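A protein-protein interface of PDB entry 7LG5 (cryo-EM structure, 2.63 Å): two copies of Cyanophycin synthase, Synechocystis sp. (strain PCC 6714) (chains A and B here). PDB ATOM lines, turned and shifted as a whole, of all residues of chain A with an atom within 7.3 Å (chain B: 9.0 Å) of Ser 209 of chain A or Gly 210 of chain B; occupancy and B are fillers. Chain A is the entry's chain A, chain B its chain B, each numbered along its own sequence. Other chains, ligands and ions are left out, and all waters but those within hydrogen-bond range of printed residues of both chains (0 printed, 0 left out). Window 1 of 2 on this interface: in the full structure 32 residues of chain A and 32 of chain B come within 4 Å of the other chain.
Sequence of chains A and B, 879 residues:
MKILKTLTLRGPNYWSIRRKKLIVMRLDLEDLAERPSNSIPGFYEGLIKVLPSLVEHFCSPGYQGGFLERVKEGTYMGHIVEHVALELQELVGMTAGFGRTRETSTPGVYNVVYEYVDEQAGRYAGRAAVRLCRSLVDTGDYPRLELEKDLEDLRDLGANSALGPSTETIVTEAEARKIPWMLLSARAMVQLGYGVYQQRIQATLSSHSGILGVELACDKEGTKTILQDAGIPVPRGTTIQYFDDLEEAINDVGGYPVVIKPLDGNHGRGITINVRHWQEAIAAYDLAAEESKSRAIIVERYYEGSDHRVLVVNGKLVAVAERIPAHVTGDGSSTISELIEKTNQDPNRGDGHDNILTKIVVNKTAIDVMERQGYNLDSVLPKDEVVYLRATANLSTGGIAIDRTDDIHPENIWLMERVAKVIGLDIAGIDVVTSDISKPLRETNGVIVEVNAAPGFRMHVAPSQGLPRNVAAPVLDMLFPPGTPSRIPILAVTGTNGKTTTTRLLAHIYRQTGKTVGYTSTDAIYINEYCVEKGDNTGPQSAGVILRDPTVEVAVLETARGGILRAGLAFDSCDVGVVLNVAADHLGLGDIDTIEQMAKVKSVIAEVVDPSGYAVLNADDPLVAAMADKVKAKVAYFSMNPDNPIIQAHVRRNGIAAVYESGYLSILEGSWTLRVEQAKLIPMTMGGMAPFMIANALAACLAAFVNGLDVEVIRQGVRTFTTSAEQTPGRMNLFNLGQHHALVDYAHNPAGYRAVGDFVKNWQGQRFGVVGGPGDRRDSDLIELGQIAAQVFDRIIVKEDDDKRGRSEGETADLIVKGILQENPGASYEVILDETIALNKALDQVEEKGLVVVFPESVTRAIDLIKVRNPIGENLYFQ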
ATOM      1  N   THR A 204      -3.363 -18.158 -33.263  1.00  0.00           N
ATOM      2  CA  THR A 204      -2.262 -17.211 -33.245  1.00  0.00           C
ATOM      3  C   THR A 204      -1.450 -17.167 -31.941  1.00  0.00           C
ATOM      4  O   THR A 204      -0.628 -16.274 -31.747  1.00  0.00           O
ATOM      5  CB  THR A 204      -2.826 -15.859 -33.681  1.00  0.00           C
ATOM      6  OG1 THR A 204      -3.971 -15.547 -32.849  1.00  0.00           O
ATOM      7  CG2 THR A 204      -3.241 -15.976 -35.123  1.00  0.00           C
ATOM      8  N   LEU A 205      -1.708 -18.108 -31.033  1.00  0.00           N
ATOM      9  CA  LEU A 205      -0.932 -18.300 -29.807  1.00  0.00           C
ATOM     10  C   LEU A 205      -0.039 -19.508 -29.983  1.00  0.00           C
ATOM     11  O   LEU A 205      -0.396 -20.465 -30.665  1.00  0.00           O
ATOM     12  CB  LEU A 205      -1.798 -18.506 -28.553  1.00  0.00           C
ATOM     13  CG  LEU A 205      -2.680 -17.358 -28.074  1.00  0.00           C
ATOM     14  CD1 LEU A 205      -3.545 -17.851 -26.951  1.00  0.00           C
ATOM     15  CD2 LEU A 205      -1.804 -16.222 -27.546  1.00  0.00           C
ATOM     16  N   SER A 206       1.107 -19.502 -29.343  1.00  0.00           N
ATOM     17  CA  SER A 206       1.999 -20.646 -29.436  1.00  0.00           C
ATOM     18  C   SER A 206       2.652 -20.958 -28.124  1.00  0.00           C
ATOM     19  O   SER A 206       2.502 -20.244 -27.136  1.00  0.00           O
ATOM     20  CB  SER A 206       3.089 -20.411 -30.457  1.00  0.00           C
ATOM     21  OG  SER A 206       4.023 -19.486 -29.997  1.00  0.00           O
ATOM     22  N   SER A 207       3.447 -22.002 -28.144  1.00  0.00           N
ATOM     23  CA  SER A 207       4.243 -22.476 -27.028  1.00  0.00           C
ATOM     24  C   SER A 207       5.284 -21.449 -26.544  1.00  0.00           C
ATOM     25  O   SER A 207       5.840 -21.596 -25.458  1.00  0.00           O
ATOM     26  CB  SER A 207       4.917 -23.759 -27.447  1.00  0.00           C
ATOM     27  OG  SER A 207       5.737 -23.500 -28.548  1.00  0.00           O
ATOM     28  N   HIS A 208       5.549 -20.409 -27.347  1.00  0.00           N
ATOM     29  CA  HIS A 208       6.471 -19.327 -27.007  1.00  0.00           C
ATOM     30  C   HIS A 208       5.775 -18.074 -26.461  1.00  0.00           C
ATOM     31  O   HIS A 208       6.444 -17.098 -26.111  1.00  0.00           O
ATOM     32  CB  HIS A 208       7.270 -18.904 -28.240  1.00  0.00           C
ATOM     33  CG  HIS A 208       8.284 -19.868 -28.700  1.00  0.00           C
ATOM     34  ND1 HIS A 208       9.622 -19.637 -28.558  1.00  0.00           N
ATOM     35  CD2 HIS A 208       8.179 -21.080 -29.255  1.00  0.00           C
ATOM     36  CE1 HIS A 208      10.292 -20.654 -29.037  1.00  0.00           C
ATOM     37  NE2 HIS A 208       9.446 -21.539 -29.460  1.00  0.00           N
ATOM     38  N   SER A 209       4.450 -18.089 -26.366  1.00  0.00           N
ATOM     39  CA  SER A 209       3.722 -16.925 -25.894  1.00  0.00           C
ATOM     40  C   SER A 209       3.510 -17.022 -24.401  1.00  0.00           C
ATOM     41  O   SER A 209       2.910 -17.993 -23.928  1.00  0.00           O
ATOM     42  CB  SER A 209       2.375 -16.796 -26.587  1.00  0.00           C
ATOM     43  OG  SER A 209       2.523 -16.564 -27.968  1.00  0.00           O
ATOM     44  N   GLY A 210       4.057 -16.055 -23.670  1.00  0.00           N
ATOM     45  CA  GLY A 210       3.996 -16.042 -22.221  1.00  0.00           C
ATOM     46  C   GLY A 210       2.693 -15.495 -21.717  1.00  0.00           C
ATOM     47  O   GLY A 210       2.119 -14.588 -22.319  1.00  0.00           O
ATOM     48  N   ILE A 211       2.301 -15.960 -20.554  1.00  0.00           N
ATOM     49  CA  ILE A 211       1.075 -15.511 -19.940  1.00  0.00           C
ATOM     50  C   ILE A 211       1.121 -14.100 -19.383  1.00  0.00           C
ATOM     51  O   ILE A 211       0.111 -13.412 -19.410  1.00  0.00           O
ATOM     52  CB  ILE A 211       0.562 -16.526 -18.895  1.00  0.00           C
ATOM     53  CG1 ILE A 211      -0.893 -16.171 -18.571  1.00  0.00           C
ATOM     54  CG2 ILE A 211       1.435 -16.601 -17.659  1.00  0.00           C
ATOM     55  CD1 ILE A 211      -1.645 -17.197 -17.843  1.00  0.00           C
ATOM     56  N   LEU A 212       2.256 -13.653 -18.855  1.00  0.00           N
ATOM     57  CA  LEU A 212       2.269 -12.322 -18.274  1.00  0.00           C
ATOM     58  C   LEU A 212       2.070 -11.271 -19.359  1.00  0.00           C
ATOM     59  O   LEU A 212       1.359 -10.287 -19.150  1.00  0.00           O
ATOM     60  CB  LEU A 212       3.594 -12.049 -17.528  1.00  0.00           C
ATOM     61  CG  LEU A 212       3.914 -12.901 -16.236  1.00  0.00           C
ATOM     62  CD1 LEU A 212       5.297 -12.541 -15.726  1.00  0.00           C
ATOM     63  CD2 LEU A 212       2.910 -12.677 -15.165  1.00  0.00           C
ATOM     64  N   GLY A 213       2.674 -11.497 -20.528  1.00  0.00           N
ATOM     65  CA  GLY A 213       2.573 -10.605 -21.675  1.00  0.00           C
ATOM     66  C   GLY A 213       1.160 -10.558 -22.219  1.00  0.00           C
ATOM     67  O   GLY A 213       0.617  -9.482 -22.474  1.00  0.00           O
ATOM     68  N   VAL A 214       0.542 -11.730 -22.383  1.00  0.00           N
ATOM     69  CA  VAL A 214      -0.799 -11.791 -22.924  1.00  0.00           C
ATOM     70  C   VAL A 214      -1.793 -11.137 -21.984  1.00  0.00           C
ATOM     71  O   VAL A 214      -2.678 -10.427 -22.446  1.00  0.00           O
ATOM     72  CB  VAL A 214      -1.218 -13.240 -23.247  1.00  0.00           C
ATOM     73  CG1 VAL A 214      -2.684 -13.289 -23.646  1.00  0.00           C
ATOM     74  CG2 VAL A 214      -0.369 -13.784 -24.382  1.00  0.00           C
ATOM     75  N   GLY A 424       6.138  -7.473 -23.657  1.00  0.00           N
ATOM     76  CA  GLY A 424       6.359  -8.899 -23.608  1.00  0.00           C
ATOM     77  C   GLY A 424       5.628  -9.942 -24.425  1.00  0.00           C
ATOM     78  O   GLY A 424       5.411 -11.055 -23.949  1.00  0.00           O
ATOM     79  N   LEU A 425       5.289  -9.571 -25.662  1.00  0.00           N
ATOM     80  CA  LEU A 425       4.523 -10.469 -26.558  1.00  0.00           C
ATOM     81  C   LEU A 425       5.324 -10.818 -27.801  1.00  0.00           C
ATOM     82  O   LEU A 425       5.875  -9.893 -28.404  1.00  0.00           O
ATOM     83  CB  LEU A 425       3.352  -9.661 -27.109  1.00  0.00           C
ATOM     84  CG  LEU A 425       2.153  -9.521 -26.187  1.00  0.00           C
ATOM     85  CD1 LEU A 425       1.138  -8.592 -26.817  1.00  0.00           C
ATOM     86  CD2 LEU A 425       1.551 -10.887 -25.936  1.00  0.00           C
ATOM     87  N   ASP A 426       5.380 -12.097 -28.174  1.00  0.00           N
ATOM     88  CA  ASP A 426       6.026 -12.429 -29.439  1.00  0.00           C
ATOM     89  C   ASP A 426       5.262 -12.057 -30.694  1.00  0.00           C
ATOM     90  O   ASP A 426       5.732 -11.233 -31.469  1.00  0.00           O
ATOM     91  CB  ASP A 426       6.410 -13.906 -29.431  1.00  0.00           C
ATOM     92  CG  ASP A 426       5.249 -14.828 -29.205  1.00  0.00           C
ATOM     93  OD1 ASP A 426       4.198 -14.357 -28.729  1.00  0.00           O
ATOM     94  OD2 ASP A 426       5.370 -15.978 -29.516  1.00  0.00           O
ATOM     95  N   ILE A 427       4.047 -12.547 -30.837  1.00  0.00           N
ATOM     96  CA  ILE A 427       3.282 -12.150 -32.005  1.00  0.00           C
ATOM     97  C   ILE A 427       2.278 -11.102 -31.572  1.00  0.00           C
ATOM     98  O   ILE A 427       1.368 -11.375 -30.775  1.00  0.00           O
ATOM     99  CB  ILE A 427       2.578 -13.324 -32.699  1.00  0.00           C
ATOM    100  CG1 ILE A 427       3.622 -14.342 -33.113  1.00  0.00           C
ATOM    101  CG2 ILE A 427       1.845 -12.792 -33.939  1.00  0.00           C
ATOM    102  CD1 ILE A 427       3.091 -15.646 -33.605  1.00  0.00           C
ATOM    103  N   ALA A 453      -2.622  -8.979 -28.422  1.00  0.00           N
ATOM    104  CA  ALA A 453      -1.937 -10.251 -28.419  1.00  0.00           C
ATOM    105  C   ALA A 453      -2.658 -11.158 -29.380  1.00  0.00           C
ATOM    106  O   ALA A 453      -3.883 -11.132 -29.432  1.00  0.00           O
ATOM    107  CB  ALA A 453      -1.908 -10.865 -27.030  1.00  0.00           C
ATOM    108  N   ALA A 454      -1.925 -12.008 -30.087  1.00  0.00           N
ATOM    109  CA  ALA A 454      -2.536 -13.013 -30.964  1.00  0.00           C
ATOM    110  C   ALA A 454      -3.512 -12.462 -32.034  1.00  0.00           C
ATOM    111  O   ALA A 454      -4.620 -12.987 -32.147  1.00  0.00           O
ATOM    112  CB  ALA A 454      -3.286 -14.002 -30.094  1.00  0.00           C
ATOM    113  N   MET A 478      10.658 -18.900 -36.059  1.00  0.00           N
ATOM    114  CA  MET A 478      11.038 -18.748 -34.663  1.00  0.00           C
ATOM    115  C   MET A 478      10.819 -20.067 -33.941  1.00  0.00           C
ATOM    116  O   MET A 478      11.562 -20.403 -33.023  1.00  0.00           O
ATOM    117  CB  MET A 478      10.293 -17.615 -33.937  1.00  0.00           C
ATOM    118  CG  MET A 478       8.889 -17.909 -33.533  1.00  0.00           C
ATOM    119  SD  MET A 478       8.083 -16.596 -32.696  1.00  0.00           S
ATOM    120  CE  MET A 478       6.516 -17.397 -32.536  1.00  0.00           C
ATOM    121  N   LEU B 205       4.077 -17.162 -11.112  1.00  0.00           N
ATOM    122  CA  LEU B 205       4.139 -17.135 -12.574  1.00  0.00           C
ATOM    123  C   LEU B 205       5.356 -16.338 -12.991  1.00  0.00           C
ATOM    124  O   LEU B 205       5.751 -15.388 -12.320  1.00  0.00           O
ATOM    125  CB  LEU B 205       2.897 -16.518 -13.236  1.00  0.00           C
ATOM    126  CG  LEU B 205       1.557 -17.233 -13.089  1.00  0.00           C
ATOM    127  CD1 LEU B 205       0.480 -16.362 -13.668  1.00  0.00           C
ATOM    128  CD2 LEU B 205       1.587 -18.546 -13.872  1.00  0.00           C
ATOM    129  N   SER B 206       5.938 -16.681 -14.118  1.00  0.00           N
ATOM    130  CA  SER B 206       7.088 -15.935 -14.599  1.00  0.00           C
ATOM    131  C   SER B 206       7.053 -15.745 -16.085  1.00  0.00           C
ATOM    132  O   SER B 206       6.188 -16.260 -16.787  1.00  0.00           O
ATOM    133  CB  SER B 206       8.382 -16.634 -14.248  1.00  0.00           C
ATOM    134  OG  SER B 206       8.566 -17.777 -15.022  1.00  0.00           O
ATOM    135  N   SER B 207       8.056 -15.051 -16.570  1.00  0.00           N
ATOM    136  CA  SER B 207       8.288 -14.777 -17.976  1.00  0.00           C
ATOM    137  C   SER B 207       8.510 -16.051 -18.814  1.00  0.00           C
ATOM    138  O   SER B 207       8.454 -16.003 -20.040  1.00  0.00           O
ATOM    139  CB  SER B 207       9.480 -13.857 -18.081  1.00  0.00           C
ATOM    140  OG  SER B 207      10.592 -14.492 -17.523  1.00  0.00           O
ATOM    141  N   HIS B 208       8.761 -17.190 -18.156  1.00  0.00           N
ATOM    142  CA  HIS B 208       8.941 -18.488 -18.805  1.00  0.00           C
ATOM    143  C   HIS B 208       7.679 -19.360 -18.800  1.00  0.00           C
ATOM    144  O   HIS B 208       7.691 -20.468 -19.341  1.00  0.00           O
ATOM    145  CB  HIS B 208      10.046 -19.282 -18.106  1.00  0.00           C
ATOM    146  CG  HIS B 208      11.415 -18.782 -18.317  1.00  0.00           C
ATOM    147  ND1 HIS B 208      12.321 -19.451 -19.090  1.00  0.00           N
ATOM    148  CD2 HIS B 208      12.035 -17.670 -17.907  1.00  0.00           C
ATOM    149  CE1 HIS B 208      13.446 -18.783 -19.115  1.00  0.00           C
ATOM    150  NE2 HIS B 208      13.300 -17.705 -18.413  1.00  0.00           N
ATOM    151  N   SER B 209       6.589 -18.874 -18.217  1.00  0.00           N
ATOM    152  CA  SER B 209       5.370 -19.659 -18.140  1.00  0.00           C
ATOM    153  C   SER B 209       4.484 -19.349 -19.325  1.00  0.00           C
ATOM    154  O   SER B 209       4.111 -18.188 -19.525  1.00  0.00           O
ATOM    155  CB  SER B 209       4.609 -19.376 -16.855  1.00  0.00           C
ATOM    156  OG  SER B 209       5.339 -19.779 -15.721  1.00  0.00           O
ATOM    157  N   GLY B 210       4.211 -20.368 -20.132  1.00  0.00           N
ATOM    158  CA  GLY B 210       3.429 -20.219 -21.345  1.00  0.00           C
ATOM    159  C   GLY B 210       1.955 -20.224 -21.067  1.00  0.00           C
ATOM    160  O   GLY B 210       1.488 -20.928 -20.173  1.00  0.00           O
ATOM    161  N   ILE B 211       1.221 -19.540 -21.915  1.00  0.00           N
ATOM    162  CA  ILE B 211      -0.214 -19.471 -21.780  1.00  0.00           C
ATOM    163  C   ILE B 211      -0.949 -20.748 -22.144  1.00  0.00           C
ATOM    164  O   ILE B 211      -1.974 -21.039 -21.545  1.00  0.00           O
ATOM    165  CB  ILE B 211      -0.790 -18.244 -22.519  1.00  0.00           C
ATOM    166  CG1 ILE B 211      -2.228 -18.035 -22.032  1.00  0.00           C
ATOM    167  CG2 ILE B 211      -0.697 -18.357 -24.028  1.00  0.00           C
ATOM    168  CD1 ILE B 211      -2.830 -16.745 -22.378  1.00  0.00           C
ATOM    169  N   LEU B 212      -0.473 -21.509 -23.123  1.00  0.00           N
ATOM    170  CA  LEU B 212      -1.221 -22.697 -23.498  1.00  0.00           C
ATOM    171  C   LEU B 212      -1.198 -23.713 -22.362  1.00  0.00           C
ATOM    172  O   LEU B 212      -2.209 -24.361 -22.087  1.00  0.00           O
ATOM    173  CB  LEU B 212      -0.643 -23.341 -24.778  1.00  0.00           C
ATOM    174  CG  LEU B 212      -0.744 -22.533 -26.132  1.00  0.00           C
ATOM    175  CD1 LEU B 212      -0.032 -23.302 -27.231  1.00  0.00           C
ATOM    176  CD2 LEU B 212      -2.154 -22.285 -26.524  1.00  0.00           C
ATOM    177  N   GLY B 213      -0.054 -23.827 -21.685  1.00  0.00           N
ATOM    178  CA  GLY B 213       0.133 -24.734 -20.562  1.00  0.00           C
ATOM    179  C   GLY B 213      -0.727 -24.339 -19.379  1.00  0.00           C
ATOM    180  O   GLY B 213      -1.403 -25.178 -18.781  1.00  0.00           O
ATOM    181  N   VAL B 214      -0.724 -23.047 -19.043  1.00  0.00           N
ATOM    182  CA  VAL B 214      -1.490 -22.575 -17.910  1.00  0.00           C
ATOM    183  C   VAL B 214      -2.978 -22.746 -18.151  1.00  0.00           C
ATOM    184  O   VAL B 214      -3.692 -23.143 -17.240  1.00  0.00           O
ATOM    185  CB  VAL B 214      -1.153 -21.110 -17.565  1.00  0.00           C
ATOM    186  CG1 VAL B 214      -2.094 -20.591 -16.489  1.00  0.00           C
ATOM    187  CG2 VAL B 214       0.278 -21.010 -17.071  1.00  0.00           C
ATOM    188  N   GLU B 215      -3.476 -22.426 -19.351  1.00  0.00           N
ATOM    189  CA  GLU B 215      -4.892 -22.629 -19.603  1.00  0.00           C
ATOM    190  C   GLU B 215      -5.291 -24.097 -19.602  1.00  0.00           C
ATOM    191  O   GLU B 215      -6.333 -24.439 -19.060  1.00  0.00           O
ATOM    192  CB  GLU B 215      -5.332 -22.010 -20.908  1.00  0.00           C
ATOM    193  CG  GLU B 215      -5.373 -20.510 -20.930  1.00  0.00           C
ATOM    194  CD  GLU B 215      -5.913 -19.972 -22.237  1.00  0.00           C
ATOM    195  OE1 GLU B 215      -6.015 -20.726 -23.197  1.00  0.00           O
ATOM    196  OE2 GLU B 215      -6.248 -18.811 -22.277  1.00  0.00           O
ATOM    197  N   LEU B 216      -4.458 -24.994 -20.136  1.00  0.00           N
ATOM    198  CA  LEU B 216      -4.799 -26.409 -20.136  1.00  0.00           C
ATOM    199  C   LEU B 216      -4.905 -26.926 -18.719  1.00  0.00           C
ATOM    200  O   LEU B 216      -5.837 -27.644 -18.393  1.00  0.00           O
ATOM    201  CB  LEU B 216      -3.749 -27.227 -20.899  1.00  0.00           C
ATOM    202  CG  LEU B 216      -3.954 -28.788 -21.007  1.00  0.00           C
ATOM    203  CD1 LEU B 216      -5.256 -29.149 -21.739  1.00  0.00           C
ATOM    204  CD2 LEU B 216      -2.754 -29.371 -21.707  1.00  0.00           C
ATOM    205  N   ALA B 217      -4.011 -26.491 -17.843  1.00  0.00           N
ATOM    206  CA  ALA B 217      -3.989 -26.915 -16.450  1.00  0.00           C
ATOM    207  C   ALA B 217      -5.236 -26.472 -15.677  1.00  0.00           C
ATOM    208  O   ALA B 217      -5.478 -26.945 -14.571  1.00  0.00           O
ATOM    209  CB  ALA B 217      -2.749 -26.372 -15.757  1.00  0.00           C
ATOM    210  N   ILE B 423       1.780 -31.613 -19.914  1.00  0.00           N
ATOM    211  CA  ILE B 423       0.892 -30.460 -19.801  1.00  0.00           C
ATOM    212  C   ILE B 423       1.557 -29.113 -20.071  1.00  0.00           C
ATOM    213  O   ILE B 423       0.891 -28.082 -20.030  1.00  0.00           O
ATOM    214  CB  ILE B 423       0.405 -30.237 -18.352  1.00  0.00           C
ATOM    215  CG1 ILE B 423      -0.419 -31.477 -17.861  1.00  0.00           C
ATOM    216  CG2 ILE B 423      -0.414 -28.918 -18.213  1.00  0.00           C
ATOM    217  CD1 ILE B 423      -1.642 -31.862 -18.682  1.00  0.00           C
ATOM    218  N   GLY B 424       2.856 -29.092 -20.346  1.00  0.00           N
ATOM    219  CA  GLY B 424       3.503 -27.835 -20.640  1.00  0.00           C
ATOM    220  C   GLY B 424       3.701 -26.689 -19.673  1.00  0.00           C
ATOM    221  O   GLY B 424       3.678 -25.529 -20.082  1.00  0.00           O
ATOM    222  N   LEU B 425       3.926 -27.036 -18.405  1.00  0.00           N
ATOM    223  CA  LEU B 425       4.085 -26.020 -17.337  1.00  0.00           C
ATOM    224  C   LEU B 425       5.466 -26.095 -16.708  1.00  0.00           C
ATOM    225  O   LEU B 425       5.882 -27.210 -16.375  1.00  0.00           O
ATOM    226  CB  LEU B 425       3.154 -26.418 -16.196  1.00  0.00           C
ATOM    227  CG  LEU B 425       1.694 -26.039 -16.370  1.00  0.00           C
ATOM    228  CD1 LEU B 425       0.885 -26.614 -15.227  1.00  0.00           C
ATOM    229  CD2 LEU B 425       1.568 -24.533 -16.417  1.00  0.00           C
ATOM    230  N   ASP B 426       6.144 -24.959 -16.541  1.00  0.00           N
ATOM    231  CA  ASP B 426       7.407 -24.999 -15.813  1.00  0.00           C
ATOM    232  C   ASP B 426       7.306 -25.201 -14.315  1.00  0.00           C
ATOM    233  O   ASP B 426       7.779 -26.209 -13.804  1.00  0.00           O
ATOM    234  CB  ASP B 426       8.222 -23.756 -16.159  1.00  0.00           C
ATOM    235  CG  ASP B 426       7.512 -22.469 -15.860  1.00  0.00           C
ATOM    236  OD1 ASP B 426       6.277 -22.494 -15.693  1.00  0.00           O
ATOM    237  OD2 ASP B 426       8.165 -21.470 -15.767  1.00  0.00           O
ATOM    238  N   ILE B 427       6.587 -24.335 -13.629  1.00  0.00           N
ATOM    239  CA  ILE B 427       6.433 -24.551 -12.202  1.00  0.00           C
ATOM    240  C   ILE B 427       5.056 -25.136 -11.966  1.00  0.00           C
ATOM    241  O   ILE B 427       4.030 -24.486 -12.219  1.00  0.00           O
ATOM    242  CB  ILE B 427       6.634 -23.280 -11.368  1.00  0.00           C
ATOM    243  CG1 ILE B 427       8.023 -22.736 -11.637  1.00  0.00           C
ATOM    244  CG2 ILE B 427       6.494 -23.641  -9.882  1.00  0.00           C
ATOM    245  CD1 ILE B 427       8.306 -21.383 -11.077  1.00  0.00           C
ATOM    246  N   ALA B 453      -1.145 -25.096 -11.995  1.00  0.00           N
ATOM    247  CA  ALA B 453      -0.162 -24.150 -12.467  1.00  0.00           C
ATOM    248  C   ALA B 453       0.069 -23.146 -11.370  1.00  0.00           C
ATOM    249  O   ALA B 453      -0.881 -22.748 -10.705  1.00  0.00           O
ATOM    250  CB  ALA B 453      -0.623 -23.452 -13.735  1.00  0.00           C
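The backbone carbonyl oxygen (O) of Ser 209 of chain A is in hydrogen-bond range of the backbone NH (N) of Ile 211 of chain B (3.0 Å).
The backbone carbonyl oxygen (O) of Ser 209 of chain B is in hydrogen-bond range of the backbone NH (N) of Ile 211 of chain A (3.0 Å).
The backbone NH (N) of His 208 of chain A lies close to the side-chain hydroxyl (OG) of Ser 206 of chain A (3.2 Å).
OG of Ser 209 of chain A is in hydrogen-bond range of OD1 of Asp 426 of chain A (2.9 Å).
The backbone NH (N) of His 208 of chain B lies close to the side-chain hydroxyl (OG) of Ser 206 of chain B, 3.2 Å away.
OD1 of Asp 426 of chain B sits at hydrogen-bond distance from OG of Ser 209 of chain B, 2.9 Å away.
Among the printed residues, merely in contact across the chains: Ser 206 of chain A with Leu 212 of chain B (3.7 Å), Ser 207 of chain A with Leu 212 of chain B (3.8 Å), Ser 209 of chain A with Gly 210 of chain B (3.4 Å), Gly 210 of chain A with Ser 209 of chain B (3.4 Å), Ile 211 of chain A with Ile 211 of chain B (3.98 Å), Ile 211 of chain A with Val 214 of chain B (3.7 Å), Leu 212 of chain A with Ser 206 of chain B (3.7 Å), Leu 212 of chain A with Ser 207 of chain B (3.8 Å) and Val 214 of chain A with Ile 211 of chain B (3.7 Å).
Ser 209 of chain A touches just these residues of chain B: Gly 210 (3.4 Å) and Ile 211 (3.0 Å).
Of chain B, only Ser 209 (3.4 Å) comes within 4 Å of Gly 210 of chain A.
Printed residues of chain B within 4 Å of Ile 211 of chain A: Ser 209, Ile 211 and Val 214.
Gly 424 of chain A touches none of the printed residues of chain B.
Printed residues of chain A within 4 Å of Ser 207 of chain B: Leu 212 (3.8 Å).
Of chain A, only Ser 209 (3.4 Å) comes within 4 Å of Gly 210 of chain B.
Of the printed residues of chain A, Leu 212 of chain B touches Ser 206 and Ser 207.
Printed residues of chain A within 4 Å of Val 214 of chain B: Ile 211.
Leu 216 of chain B touches none of the printed residues of chain A.
The nearest printed residue of chain A that does not touch Gly 210 of chain B is Gly 210 of chain A (4.3 Å).
The nearest printed residue of chain A that does not touch Val 214 of chain B is Gly 210 of chain A (7.6 Å).
Of the 18 printed residues of chain A, 7 touch a printed residue of chain B.
Printed residues of chain A that touch a printed residue of chain B: Ser 206, Ser 207, Ser 209, Gly 210, Ile 211, Leu 212 and Val 214.
Hydrophobic or aromatic side chains of chain B that line the printed part of chain A: Ile 211, Leu 212 and Val 214.
Among the printed residues, no Asp or Glu carboxylate lies within 4 Å of a Lys or Arg side-chain nitrogen of the other chain.
Ser 207 of chain A touches Leu 212 of chain B, and with the chains exchanged Leu 212 of chain A touches Ser 207 of chain B.
Ser 209 of chain A touches Gly 210 of chain B, and with the chains exchanged Gly 210 of chain A touches Ser 209 of chain B.
Ser 209 of chain A touches Ile 211 of chain B, and with the chains exchanged Ile 211 of chain A touches Ser 209 of chain B.
Ile 211 of chain A touches Val 214 of chain B, and with the chains exchanged Val 214 of chain A touches Ile 211 of chain B.
Of the 11 pairs that touch across the chains among the printed residues, 11 have their exchanged pair printed and touching as well.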
